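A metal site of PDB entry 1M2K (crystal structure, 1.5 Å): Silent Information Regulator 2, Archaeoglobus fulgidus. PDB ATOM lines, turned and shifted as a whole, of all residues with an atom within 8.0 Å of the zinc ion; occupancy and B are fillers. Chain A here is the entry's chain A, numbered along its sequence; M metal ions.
The side-chain sulfur (SG) of Cys 124 sits close to the side-chain hydroxyl (OG) of Ser 126 (3.3 Å). SG of Cys 148 sits close to OG of Ser 126 (3.6 Å). The side-chain sulfur of Cys 145 lies close to the backbone NH of Lys 147 (3.3 Å). O of Asn 129 lies within hydrogen-bond range of N of Cys 124 (2.9 Å). N of Cys 145 lies within hydrogen-bond range of O of Ser 150, 2.8 Å away.
The zinc ion is bound by SG of Cys 124 (2.3 Å), SG of Cys 127 (2.3 Å), SG of Cys 145 (2.3 Å) and SG of Cys 148 (2.3 Å).
Four residues have an atom within 4 Å of the zinc ion: Cys 124, Cys 127, Cys 145 and Cys 148. The nearest printed residue that does not touch the zinc ion is Ser 126 (4.1 Å).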
ATOM      1  N   ARG A 123      22.108  -7.796   8.427  1.00  0.00           N
ATOM      2  CA  ARG A 123      20.658  -7.695   8.369  1.00  0.00           C
ATOM      3  C   ARG A 123      20.021  -7.509   9.736  1.00  0.00           C
ATOM      4  O   ARG A 123      20.635  -7.780  10.768  1.00  0.00           O
ATOM      5  CB  ARG A 123      20.068  -8.924   7.674  1.00  0.00           C
ATOM      6  CG  ARG A 123      20.301 -10.244   8.399  1.00  0.00           C
ATOM      7  CD  ARG A 123      19.919 -11.412   7.508  1.00  0.00           C
ATOM      8  NE  ARG A 123      19.956 -12.695   8.200  1.00  0.00           N
ATOM      9  CZ  ARG A 123      19.079 -13.062   9.136  1.00  0.00           C
ATOM     10  NH1 ARG A 123      18.106 -12.242   9.491  1.00  0.00           N
ATOM     11  NH2 ARG A 123      19.189 -14.252   9.714  1.00  0.00           N
ATOM     12  N   CYS A 124      18.792  -7.030   9.735  1.00  0.00           N
ATOM     13  CA  CYS A 124      18.069  -6.795  10.976  1.00  0.00           C
ATOM     14  C   CYS A 124      17.550  -8.106  11.524  1.00  0.00           C
ATOM     15  O   CYS A 124      17.168  -9.006  10.778  1.00  0.00           O
ATOM     16  CB  CYS A 124      16.905  -5.841  10.725  1.00  0.00           C
ATOM     17  SG  CYS A 124      16.001  -5.396  12.236  1.00  0.00           S
ATOM     18  N   THR A 125      17.543  -8.222  12.853  1.00  0.00           N
ATOM     19  CA  THR A 125      17.080  -9.438  13.517  1.00  0.00           C
ATOM     20  C   THR A 125      15.554  -9.546  13.536  1.00  0.00           C
ATOM     21  O   THR A 125      15.003 -10.613  13.793  1.00  0.00           O
ATOM     22  CB  THR A 125      17.598  -9.520  14.964  1.00  0.00           C
ATOM     23  OG1 THR A 125      17.249  -8.312  15.651  1.00  0.00           O
ATOM     24  CG2 THR A 125      19.113  -9.689  14.975  1.00  0.00           C
ATOM     25  N   SER A 126      14.877  -8.434  13.260  1.00  0.00           N
ATOM     26  CA  SER A 126      13.413  -8.428  13.271  1.00  0.00           C
ATOM     27  C   SER A 126      12.783  -8.113  11.917  1.00  0.00           C
ATOM     28  O   SER A 126      12.126  -8.977  11.325  1.00  0.00           O
ATOM     29  CB  SER A 126      12.900  -7.453  14.328  1.00  0.00           C
ATOM     30  OG  SER A 126      13.422  -6.157  14.140  1.00  0.00           O
ATOM     31  N   CYS A 127      12.956  -6.889  11.427  1.00  0.00           N
ATOM     32  CA  CYS A 127      12.368  -6.506  10.155  1.00  0.00           C
ATOM     33  C   CYS A 127      13.152  -7.037   8.960  1.00  0.00           C
ATOM     34  O   CYS A 127      14.336  -7.359   9.076  1.00  0.00           O
ATOM     35  CB  CYS A 127      12.245  -4.971  10.055  1.00  0.00           C
ATOM     36  SG  CYS A 127      13.761  -4.087   9.555  1.00  0.00           S
ATOM     37  N   ASN A 128      12.474  -7.138   7.820  1.00  0.00           N
ATOM     38  CA  ASN A 128      13.086  -7.627   6.599  1.00  0.00           C
ATOM     39  C   ASN A 128      13.931  -6.551   5.951  1.00  0.00           C
ATOM     40  O   ASN A 128      13.514  -5.895   4.996  1.00  0.00           O
ATOM     41  CB  ASN A 128      12.010  -8.090   5.608  1.00  0.00           C
ATOM     42  CG  ASN A 128      11.284  -9.327   6.070  1.00  0.00           C
ATOM     43  OD1 ASN A 128      10.689  -9.356   7.155  1.00  0.00           O
ATOM     44  ND2 ASN A 128      11.321 -10.381   5.258  1.00  0.00           N
ATOM     45  N   ASN A 129      15.140  -6.352   6.481  1.00  0.00           N
ATOM     46  CA  ASN A 129      16.045  -5.345   5.943  1.00  0.00           C
ATOM     47  C   ASN A 129      17.490  -5.814   6.036  1.00  0.00           C
ATOM     48  O   ASN A 129      17.948  -6.283   7.078  1.00  0.00           O
ATOM     49  CB  ASN A 129      15.885  -4.024   6.701  1.00  0.00           C
ATOM     50  CG  ASN A 129      16.727  -2.912   6.100  1.00  0.00           C
ATOM     51  OD1 ASN A 129      16.573  -2.572   4.928  1.00  0.00           O
ATOM     52  ND2 ASN A 129      17.620  -2.346   6.899  1.00  0.00           N
ATOM     53  N   SER A 130      18.213  -5.696   4.924  1.00  0.00           N
ATOM     54  CA  SER A 130      19.599  -6.099   4.865  1.00  0.00           C
ATOM     55  C   SER A 130      20.337  -5.206   3.871  1.00  0.00           C
ATOM     56  O   SER A 130      19.723  -4.603   2.990  1.00  0.00           O
ATOM     57  CB  SER A 130      19.727  -7.550   4.418  1.00  0.00           C
ATOM     58  OG  SER A 130      19.349  -7.713   3.071  1.00  0.00           O
ATOM     59  N   LYS A 144      22.803  -1.230  15.271  1.00  0.00           N
ATOM     60  CA  LYS A 144      21.345  -1.153  15.321  1.00  0.00           C
ATOM     61  C   LYS A 144      20.737  -0.877  13.948  1.00  0.00           C
ATOM     62  O   LYS A 144      21.357  -0.219  13.108  1.00  0.00           O
ATOM     63  CB  LYS A 144      20.875  -0.058  16.289  1.00  0.00           C
ATOM     64  CG  LYS A 144      20.995  -0.390  17.756  1.00  0.00           C
ATOM     65  CD  LYS A 144      22.394  -0.126  18.265  1.00  0.00           C
ATOM     66  CE  LYS A 144      22.516  -0.464  19.746  1.00  0.00           C
ATOM     67  NZ  LYS A 144      23.885  -0.152  20.256  1.00  0.00           N
ATOM     68  N   CYS A 145      19.517  -1.360  13.742  1.00  0.00           N
ATOM     69  CA  CYS A 145      18.803  -1.161  12.485  1.00  0.00           C
ATOM     70  C   CYS A 145      18.138   0.221  12.471  1.00  0.00           C
ATOM     71  O   CYS A 145      17.407   0.565  13.389  1.00  0.00           O
ATOM     72  CB  CYS A 145      17.745  -2.242  12.294  1.00  0.00           C
ATOM     73  SG  CYS A 145      16.590  -1.958  10.918  1.00  0.00           S
ATOM     74  N   ASP A 146      18.394   0.989  11.422  1.00  0.00           N
ATOM     75  CA  ASP A 146      17.815   2.329  11.295  1.00  0.00           C
ATOM     76  C   ASP A 146      16.346   2.272  10.895  1.00  0.00           C
ATOM     77  O   ASP A 146      15.560   3.144  11.262  1.00  0.00           O
ATOM     78  CB  ASP A 146      18.605   3.149  10.270  1.00  0.00           C
ATOM     79  CG  ASP A 146      18.546   2.557   8.867  1.00  0.00           C
ATOM     80  OD1 ASP A 146      18.947   1.377   8.702  1.00  0.00           O
ATOM     81  OD2 ASP A 146      18.086   3.252   7.942  1.00  0.00           O
ATOM     82  N   LYS A 147      15.977   1.228  10.145  1.00  0.00           N
ATOM     83  CA  LYS A 147      14.597   1.052   9.705  1.00  0.00           C
ATOM     84  C   LYS A 147      13.631   1.047  10.884  1.00  0.00           C
ATOM     85  O   LYS A 147      12.681   1.829  10.939  1.00  0.00           O
ATOM     86  CB  LYS A 147      14.448  -0.252   8.931  1.00  0.00           C
ATOM     87  CG  LYS A 147      15.178  -0.290   7.591  1.00  0.00           C
ATOM     88  CD  LYS A 147      14.603   0.731   6.624  1.00  0.00           C
ATOM     89  CE  LYS A 147      15.213   0.577   5.244  1.00  0.00           C
ATOM     90  NZ  LYS A 147      16.704   0.690   5.277  1.00  0.00           N
ATOM     91  N   CYS A 148      13.893   0.152  11.839  1.00  0.00           N
ATOM     92  CA  CYS A 148      13.050   0.024  13.021  1.00  0.00           C
ATOM     93  C   CYS A 148      13.885   0.183  14.296  1.00  0.00           C
ATOM     94  O   CYS A 148      14.807   0.995  14.347  1.00  0.00           O
ATOM     95  CB  CYS A 148      12.372  -1.343  13.029  1.00  0.00           C
ATOM     96  SG  CYS A 148      13.543  -2.734  13.065  1.00  0.00           S
ATOM     97  N   GLY A 149      13.550  -0.603  15.315  1.00  0.00           N
ATOM     98  CA  GLY A 149      14.270  -0.533  16.561  1.00  0.00           C
ATOM     99  C   GLY A 149      14.714  -1.896  17.050  1.00  0.00           C
ATOM    100  O   GLY A 149      14.071  -2.509  17.897  1.00  0.00           O
ATOM    101  N   SER A 150      15.832  -2.371  16.502  1.00  0.00           N
ATOM    102  CA  SER A 150      16.374  -3.669  16.879  1.00  0.00           C
ATOM    103  C   SER A 150      17.841  -3.751  16.459  1.00  0.00           C
ATOM    104  O   SER A 150      18.340  -2.876  15.753  1.00  0.00           O
ATOM    105  CB  SER A 150      15.589  -4.792  16.197  1.00  0.00           C
ATOM    106  OG  SER A 150      14.220  -4.769  16.587  1.00  0.00           O
ATOM    107  N   LEU A 151      18.520  -4.803  16.902  1.00  0.00           N
ATOM    108  CA  LEU A 151      19.931  -4.989  16.565  1.00  0.00           C
ATOM    109  C   LEU A 151      20.132  -5.634  15.206  1.00  0.00           C
ATOM    110  O   LEU A 151      19.260  -6.346  14.704  1.00  0.00           O
ATOM    111  CB  LEU A 151      20.639  -5.842  17.626  1.00  0.00           C
ATOM    112  CG  LEU A 151      21.053  -5.178  18.948  1.00  0.00           C
ATOM    113  CD1 LEU A 151      19.832  -4.660  19.690  1.00  0.00           C
ATOM    114  CD2 LEU A 151      21.802  -6.193  19.783  1.00  0.00           C
ATOM    115  N   LEU A 152      21.279  -5.360  14.605  1.00  0.00           N
ATOM    116  CA  LEU A 152      21.643  -5.935  13.324  1.00  0.00           C
ATOM    117  C   LEU A 152      22.486  -7.159  13.641  1.00  0.00           C
ATOM    118  O   LEU A 152      23.041  -7.271  14.735  1.00  0.00           O
ATOM    119  CB  LEU A 152      22.473  -4.956  12.500  1.00  0.00           C
ATOM    120  CG  LEU A 152      21.759  -3.740  11.901  1.00  0.00           C
ATOM    121  CD1 LEU A 152      22.812  -2.773  11.369  1.00  0.00           C
ATOM    122  CD2 LEU A 152      20.826  -4.172  10.784  1.00  0.00           C
HETATM  123 ZN    ZN M   1      14.966  -3.522  11.423  1.00  0.00          ZN
